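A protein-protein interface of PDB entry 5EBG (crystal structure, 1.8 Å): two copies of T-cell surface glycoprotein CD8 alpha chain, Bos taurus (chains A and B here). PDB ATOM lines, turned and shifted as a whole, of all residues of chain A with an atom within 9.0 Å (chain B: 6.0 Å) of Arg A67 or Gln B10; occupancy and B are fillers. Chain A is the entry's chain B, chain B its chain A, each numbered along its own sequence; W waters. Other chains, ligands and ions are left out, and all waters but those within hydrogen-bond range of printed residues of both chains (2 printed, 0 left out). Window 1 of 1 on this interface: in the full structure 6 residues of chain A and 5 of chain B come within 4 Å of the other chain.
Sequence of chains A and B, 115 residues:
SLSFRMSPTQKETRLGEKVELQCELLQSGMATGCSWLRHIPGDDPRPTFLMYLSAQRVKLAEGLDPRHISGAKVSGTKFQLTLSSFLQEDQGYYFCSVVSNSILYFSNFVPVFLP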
ATOM      1  N   GLY A  16       2.618 -13.611 -22.458  1.00  0.00           N
ATOM      2  CA  GLY A  16       1.308 -13.783 -21.852  1.00  0.00           C
ATOM      3  C   GLY A  16       0.240 -12.825 -22.347  1.00  0.00           C
ATOM      4  O   GLY A  16      -0.908 -12.877 -21.895  1.00  0.00           O
ATOM      5  N   LEU A  60      -5.659 -24.526 -39.846  1.00  0.00           N
ATOM      6  CA  LEU A  60      -4.333 -24.355 -39.263  1.00  0.00           C
ATOM      7  C   LEU A  60      -3.336 -25.336 -39.856  1.00  0.00           C
ATOM      8  O   LEU A  60      -3.689 -26.465 -40.205  1.00  0.00           O
ATOM      9  CB  LEU A  60      -4.365 -24.534 -37.743  1.00  0.00           C
ATOM     10  CG  LEU A  60      -5.075 -23.480 -36.904  1.00  0.00           C
ATOM     11  CD1 LEU A  60      -4.882 -23.793 -35.426  1.00  0.00           C
ATOM     12  CD2 LEU A  60      -4.524 -22.104 -37.237  1.00  0.00           C
ATOM     13  N   LEU A  64       0.055 -26.946 -35.266  1.00  0.00           N
ATOM     14  CA  LEU A  64      -0.364 -25.762 -34.512  1.00  0.00           C
ATOM     15  C   LEU A  64      -1.583 -26.047 -33.633  1.00  0.00           C
ATOM     16  O   LEU A  64      -2.459 -26.835 -33.999  1.00  0.00           O
ATOM     17  CB  LEU A  64      -0.678 -24.597 -35.456  1.00  0.00           C
ATOM     18  CG  LEU A  64       0.473 -23.772 -36.034  1.00  0.00           C
ATOM     19  CD1 LEU A  64       1.434 -24.618 -36.834  1.00  0.00           C
ATOM     20  CD2 LEU A  64      -0.078 -22.637 -36.888  1.00  0.00           C
ATOM     21  N   ASP A  65      -1.630 -25.385 -32.479  1.00  0.00           N
ATOM     22  CA  ASP A  65      -2.656 -25.606 -31.465  1.00  0.00           C
ATOM     23  C   ASP A  65      -3.635 -24.437 -31.477  1.00  0.00           C
ATOM     24  O   ASP A  65      -3.236 -23.304 -31.216  1.00  0.00           O
ATOM     25  CB  ASP A  65      -1.977 -25.690 -30.095  1.00  0.00           C
ATOM     26  CG  ASP A  65      -2.893 -26.212 -29.003  1.00  0.00           C
ATOM     27  OD1 ASP A  65      -4.127 -26.049 -29.099  1.00  0.00           O
ATOM     28  OD2 ASP A  65      -2.361 -26.779 -28.029  1.00  0.00           O
ATOM     29  N   PRO A  66      -4.915 -24.708 -31.788  1.00  0.00           N
ATOM     30  CA  PRO A  66      -5.947 -23.668 -31.870  1.00  0.00           C
ATOM     31  C   PRO A  66      -6.168 -22.974 -30.534  1.00  0.00           C
ATOM     32  O   PRO A  66      -6.805 -21.920 -30.488  1.00  0.00           O
ATOM     33  CB  PRO A  66      -7.203 -24.457 -32.245  1.00  0.00           C
ATOM     34  CG  PRO A  66      -6.928 -25.840 -31.796  1.00  0.00           C
ATOM     35  CD  PRO A  66      -5.473 -26.045 -32.054  1.00  0.00           C
ATOM     36  N   ARG A  67      -5.657 -23.536 -29.468  1.00  0.00           N
ATOM     37  CA  ARG A  67      -5.763 -22.933 -28.151  1.00  0.00           C
ATOM     38  C   ARG A  67      -4.729 -21.824 -27.998  1.00  0.00           C
ATOM     39  O   ARG A  67      -4.772 -21.068 -27.075  1.00  0.00           O
ATOM     40  CB  ARG A  67      -5.517 -23.933 -27.052  1.00  0.00           C
ATOM     41  CG  ARG A  67      -6.577 -24.975 -26.920  1.00  0.00           C
ATOM     42  CD  ARG A  67      -6.639 -25.386 -25.515  1.00  0.00           C
ATOM     43  NE  ARG A  67      -5.865 -26.557 -25.302  1.00  0.00           N
ATOM     44  CZ  ARG A  67      -5.682 -27.139 -24.130  1.00  0.00           C
ATOM     45  NH1 ARG A  67      -6.225 -26.688 -23.060  1.00  0.00           N
ATOM     46  NH2 ARG A  67      -4.941 -28.176 -24.058  1.00  0.00           N
ATOM     47  N   HIS A  68      -3.794 -21.827 -28.909  1.00  0.00           N
ATOM     48  CA  HIS A  68      -2.708 -20.850 -28.876  1.00  0.00           C
ATOM     49  C   HIS A  68      -2.790 -19.893 -30.052  1.00  0.00           C
ATOM     50  O   HIS A  68      -2.575 -18.687 -29.914  1.00  0.00           O
ATOM     51  CB  HIS A  68      -1.354 -21.563 -28.911  1.00  0.00           C
ATOM     52  CG  HIS A  68      -0.182 -20.633 -28.995  1.00  0.00           C
ATOM     53  ND1 HIS A  68       0.211 -19.834 -27.944  1.00  0.00           N
ATOM     54  CD2 HIS A  68       0.695 -20.391 -30.001  1.00  0.00           C
ATOM     55  CE1 HIS A  68       1.274 -19.132 -28.299  1.00  0.00           C
ATOM     56  NE2 HIS A  68       1.585 -19.451 -29.543  1.00  0.00           N
ATOM     57  N   ILE A  69      -3.081 -20.446 -31.220  1.00  0.00           N
ATOM     58  CA  ILE A  69      -3.135 -19.643 -32.427  1.00  0.00           C
ATOM     59  C   ILE A  69      -4.386 -19.928 -33.255  1.00  0.00           C
ATOM     60  O   ILE A  69      -4.777 -21.078 -33.469  1.00  0.00           O
ATOM     61  CB  ILE A  69      -1.847 -19.786 -33.270  1.00  0.00           C
ATOM     62  CG1 ILE A  69      -1.904 -18.898 -34.516  1.00  0.00           C
ATOM     63  CG2 ILE A  69      -1.595 -21.242 -33.650  1.00  0.00           C
ATOM     64  CD1 ILE A  69      -0.575 -18.768 -35.220  1.00  0.00           C
ATOM     65  N   SER A  70      -5.027 -18.860 -33.705  1.00  0.00           N
ATOM     66  CA  SER A  70      -6.189 -18.998 -34.553  1.00  0.00           C
ATOM     67  C   SER A  70      -6.291 -17.763 -35.424  1.00  0.00           C
ATOM     68  O   SER A  70      -5.400 -16.899 -35.421  1.00  0.00           O
ATOM     69  CB  SER A  70      -7.454 -19.172 -33.708  1.00  0.00           C
ATOM     70  OG  SER A  70      -8.588 -19.426 -34.521  1.00  0.00           O
ATOM     71  N   THR A  82      -4.823 -14.349 -34.468  1.00  0.00           N
ATOM     72  CA  THR A  82      -4.768 -14.096 -33.036  1.00  0.00           C
ATOM     73  C   THR A  82      -3.875 -15.104 -32.324  1.00  0.00           C
ATOM     74  O   THR A  82      -4.017 -16.308 -32.512  1.00  0.00           O
ATOM     75  CB  THR A  82      -6.174 -14.147 -32.398  1.00  0.00           C
ATOM     76  OG1 THR A  82      -6.992 -13.101 -32.940  1.00  0.00           O
ATOM     77  CG2 THR A  82      -6.078 -13.982 -30.887  1.00  0.00           C
ATOM     78  N   LEU A  83      -2.958 -14.595 -31.509  1.00  0.00           N
ATOM     79  CA  LEU A  83      -2.232 -15.411 -30.545  1.00  0.00           C
ATOM     80  C   LEU A  83      -2.845 -15.163 -29.166  1.00  0.00           C
ATOM     81  O   LEU A  83      -3.002 -14.020 -28.751  1.00  0.00           O
ATOM     82  CB  LEU A  83      -0.754 -15.037 -30.544  1.00  0.00           C
ATOM     83  CG  LEU A  83      -0.063 -15.205 -31.897  1.00  0.00           C
ATOM     84  CD1 LEU A  83       1.266 -14.471 -31.904  1.00  0.00           C
ATOM     85  CD2 LEU A  83       0.119 -16.679 -32.233  1.00  0.00           C
ATOM     86  N   SER A  84      -3.186 -16.232 -28.452  1.00  0.00           N
ATOM     87  CA  SER A  84      -3.951 -16.096 -27.209  1.00  0.00           C
ATOM     88  C   SER A  84      -3.090 -15.721 -26.002  1.00  0.00           C
ATOM     89  O   SER A  84      -3.562 -15.090 -25.044  1.00  0.00           O
ATOM     90  CB  SER A  84      -4.706 -17.393 -26.916  1.00  0.00           C
ATOM     91  OG  SER A  84      -3.807 -18.465 -26.704  1.00  0.00           O
ATOM     92  N   SER A  85      -1.833 -16.140 -26.044  1.00  0.00           N
ATOM     93  CA  SER A  85      -0.884 -15.895 -24.968  1.00  0.00           C
ATOM     94  C   SER A  85       0.504 -15.965 -25.575  1.00  0.00           C
ATOM     95  O   SER A  85       0.967 -17.048 -25.940  1.00  0.00           O
ATOM     96  CB  SER A  85      -1.027 -16.952 -23.876  1.00  0.00           C
ATOM     97  OG  SER A  85      -0.125 -16.705 -22.806  1.00  0.00           O
ATOM     98  N   PHE A  86       1.165 -14.817 -25.697  1.00  0.00           N
ATOM     99  CA  PHE A  86       2.408 -14.748 -26.456  1.00  0.00           C
ATOM    100  C   PHE A  86       3.532 -15.509 -25.785  1.00  0.00           C
ATOM    101  O   PHE A  86       3.745 -15.403 -24.568  1.00  0.00           O
ATOM    102  CB  PHE A  86       2.839 -13.297 -26.717  1.00  0.00           C
ATOM    103  CG  PHE A  86       3.851 -13.155 -27.834  1.00  0.00           C
ATOM    104  CD1 PHE A  86       3.437 -13.051 -29.153  1.00  0.00           C
ATOM    105  CD2 PHE A  86       5.209 -13.130 -27.563  1.00  0.00           C
ATOM    106  CE1 PHE A  86       4.358 -12.916 -30.179  1.00  0.00           C
ATOM    107  CE2 PHE A  86       6.143 -13.000 -28.589  1.00  0.00           C
ATOM    108  CZ  PHE A  86       5.723 -12.893 -29.891  1.00  0.00           C
ATOM    109  N   LEU A  87       4.253 -16.272 -26.603  1.00  0.00           N
ATOM    110  CA  LEU A  87       5.403 -17.039 -26.160  1.00  0.00           C
ATOM    111  C   LEU A  87       6.661 -16.599 -26.903  1.00  0.00           C
ATOM    112  O   LEU A  87       6.594 -16.142 -28.046  1.00  0.00           O
ATOM    113  CB  LEU A  87       5.164 -18.530 -26.415  1.00  0.00           C
ATOM    114  CG  LEU A  87       3.949 -19.195 -25.761  1.00  0.00           C
ATOM    115  CD1 LEU A  87       3.704 -20.574 -26.373  1.00  0.00           C
ATOM    116  CD2 LEU A  87       4.160 -19.302 -24.264  1.00  0.00           C
ATOM    117  N   PRO B   8      -4.876 -16.377 -15.528  1.00  0.00           N
ATOM    118  CA  PRO B   8      -4.207 -17.029 -16.661  1.00  0.00           C
ATOM    119  C   PRO B   8      -4.948 -16.797 -17.967  1.00  0.00           C
ATOM    120  O   PRO B   8      -6.059 -16.268 -17.967  1.00  0.00           O
ATOM    121  CB  PRO B   8      -4.316 -18.506 -16.302  1.00  0.00           C
ATOM    122  CG  PRO B   8      -5.680 -18.586 -15.647  1.00  0.00           C
ATOM    123  CD  PRO B   8      -5.721 -17.331 -14.784  1.00  0.00           C
ATOM    124  N   THR B   9      -4.345 -17.201 -19.077  1.00  0.00           N
ATOM    125  CA  THR B   9      -4.997 -17.014 -20.371  1.00  0.00           C
ATOM    126  C   THR B   9      -5.957 -18.161 -20.691  1.00  0.00           C
ATOM    127  O   THR B   9      -6.830 -18.031 -21.556  1.00  0.00           O
ATOM    128  CB  THR B   9      -3.974 -16.855 -21.516  1.00  0.00           C
ATOM    129  OG1 THR B   9      -3.177 -18.042 -21.626  1.00  0.00           O
ATOM    130  CG2 THR B   9      -3.076 -15.642 -21.278  1.00  0.00           C
ATOM    131  N   GLN B  10      -5.780 -19.275 -19.987  1.00  0.00           N
ATOM    132  CA  GLN B  10      -6.632 -20.452 -20.121  1.00  0.00           C
ATOM    133  C   GLN B  10      -6.472 -21.274 -18.848  1.00  0.00           C
ATOM    134  O   GLN B  10      -5.497 -21.116 -18.115  1.00  0.00           O
ATOM    135  CB  GLN B  10      -6.213 -21.302 -21.330  1.00  0.00           C
ATOM    136  CG  GLN B  10      -4.890 -22.038 -21.148  1.00  0.00           C
ATOM    137  CD  GLN B  10      -4.396 -22.720 -22.414  1.00  0.00           C
ATOM    138  OE1 GLN B  10      -4.423 -22.142 -23.500  1.00  0.00           O
ATOM    139  NE2 GLN B  10      -3.917 -23.954 -22.271  1.00  0.00           N
ATOM    140  N   LYS B  11      -7.427 -22.149 -18.572  1.00  0.00           N
ATOM    141  CA  LYS B  11      -7.305 -23.003 -17.406  1.00  0.00           C
ATOM    142  C   LYS B  11      -8.034 -24.318 -17.613  1.00  0.00           C
ATOM    143  O   LYS B  11      -9.206 -24.323 -17.963  1.00  0.00           O
ATOM    144  CB  LYS B  11      -7.838 -22.291 -16.157  1.00  0.00           C
ATOM    145  CG  LYS B  11      -7.803 -23.162 -14.897  1.00  0.00           C
ATOM    146  CD  LYS B  11      -6.382 -23.588 -14.533  1.00  0.00           C
ATOM    147  CE  LYS B  11      -6.359 -24.537 -13.336  1.00  0.00           C
ATOM    148  NZ  LYS B  11      -4.999 -25.115 -13.091  1.00  0.00           N
ATOM    149  N   GLU B  12      -7.311 -25.426 -17.442  1.00  0.00           N
ATOM    150  CA  GLU B  12      -7.931 -26.734 -17.312  1.00  0.00           C
ATOM    151  C   GLU B  12      -8.086 -26.967 -15.821  1.00  0.00           C
ATOM    152  O   GLU B  12      -7.092 -27.039 -15.085  1.00  0.00           O
ATOM    153  CB  GLU B  12      -7.045 -27.831 -17.913  1.00  0.00           C
ATOM    154  CG  GLU B  12      -6.608 -27.582 -19.351  1.00  0.00           C
ATOM    155  CD  GLU B  12      -5.436 -28.465 -19.771  1.00  0.00           C
ATOM    156  OE1 GLU B  12      -4.476 -27.931 -20.375  1.00  0.00           O
ATOM    157  OE2 GLU B  12      -5.468 -29.685 -19.487  1.00  0.00           O
ATOM    158  N   VAL B 110     -11.124 -16.342 -21.584  1.00  0.00           N
ATOM    159  CA  VAL B 110     -10.330 -17.366 -20.934  1.00  0.00           C
ATOM    160  C   VAL B 110     -11.158 -18.642 -20.891  1.00  0.00           C
ATOM    161  O   VAL B 110     -12.168 -18.702 -20.201  1.00  0.00           O
ATOM    162  CB  VAL B 110      -9.999 -16.960 -19.483  1.00  0.00           C
ATOM    163  CG1 VAL B 110      -9.184 -18.039 -18.789  1.00  0.00           C
ATOM    164  CG2 VAL B 110      -9.275 -15.616 -19.454  1.00  0.00           C
ATOM    165  N   PRO B 111     -10.747 -19.665 -21.648  1.00  0.00           N
ATOM    166  CA  PRO B 111     -11.485 -20.932 -21.571  1.00  0.00           C
ATOM    167  C   PRO B 111     -11.191 -21.630 -20.256  1.00  0.00           C
ATOM    168  O   PRO B 111     -10.026 -21.871 -19.942  1.00  0.00           O
ATOM    169  CB  PRO B 111     -10.904 -21.754 -22.728  1.00  0.00           C
ATOM    170  CG  PRO B 111     -10.221 -20.767 -23.616  1.00  0.00           C
ATOM    171  CD  PRO B 111      -9.735 -19.672 -22.715  1.00  0.00           C
ATOM    172  N   VAL B 112     -12.233 -21.949 -19.494  1.00  0.00           N
ATOM    173  CA  VAL B 112     -12.058 -22.686 -18.252  1.00  0.00           C
ATOM    174  C   VAL B 112     -12.906 -23.952 -18.342  1.00  0.00           C
ATOM    175  O   VAL B 112     -14.133 -23.896 -18.258  1.00  0.00           O
ATOM    176  CB  VAL B 112     -12.460 -21.844 -17.028  1.00  0.00           C
ATOM    177  CG1 VAL B 112     -12.292 -22.643 -15.755  1.00  0.00           C
ATOM    178  CG2 VAL B 112     -11.613 -20.561 -16.960  1.00  0.00           C
HETATM  179  O   HOH W   1      -6.971 -21.253 -25.367  1.00  0.00           O
HETATM  180  O   HOH W   2      -3.576 -19.552 -23.822  1.00  0.00           O
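The side-chain carboxylate (OE1) of Glu B12 is in salt-bridge range of the guanidinium group (NH1) of Arg A67 (3.4 Å).
O of Phe A86 lies within hydrogen-bond range of N of Gly A16, 3.0 Å away. N of Arg A67 lies within hydrogen-bond range of OD1 of Asp A65 (3.0 Å). The side-chain hydroxyl (OG) of Ser A84 sits at hydrogen-bond distance from the backbone carbonyl oxygen (O) of Arg A67. The backbone NH of Ser A84 is in hydrogen-bond range of the backbone carbonyl oxygen of His A68 (2.9 Å).
Among the printed residues, pairs that only touch across the chains: Ser A85 with Thr B9, Gly A16 with Thr B9, Arg A67 with Gln B10 and Ser A84 with Thr B9.
Arg A67 touches just these residues of chain B: Gln B10 and Glu B12. Printed residues of chain A within 4 Å of Glu B12: Arg A67. Of the printed residues of chain B, Ser A85 touches Thr B9. Printed residues of chain B within 4 Å of Ser A84: Thr B9 (3.8 Å). The nearest printed residue of chain B that does not touch Arg A67 is Pro B111 (6.1 Å). The nearest residue of chain A that does not touch Gln B10 is Ser A84 (4.9 Å). The nearest printed residue of chain B that does not touch Ser A85 is Gln B10 (6.2 Å).
Of the 8 printed residues of chain B, 3 touch a printed residue of chain A. Printed residues of chain B that touch a printed residue of chain A: Thr B9, Gln B10 and Glu B12. Of the 15 printed residues of chain A, 4 touch a printed residue of chain B. Printed residues of chain A that touch a printed residue of chain B: Gly A16, Arg A67, Ser A84 and Ser A85. Among the printed residues, Asp or Glu carboxylates within 4 Å of a Lys or Arg side-chain nitrogen of the other chain: Arg A67 with Glu B12.
No position is printed for both chains. Of the 5 pairs that touch across the chains among the printed residues, none has its exchanged pair printed and touching as well.
Water W2 lies within hydrogen-bond range of OG1 of Thr B9 (2.7 Å), OE1 of Gln B10 (2.7 Å) and OG of Ser A84 (3.1 Å). Water W1 lies within hydrogen-bond range of the backbone carbonyl oxygen (O) of Arg A67 and the side-chain amide oxygen (OE1) of Gln B10.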
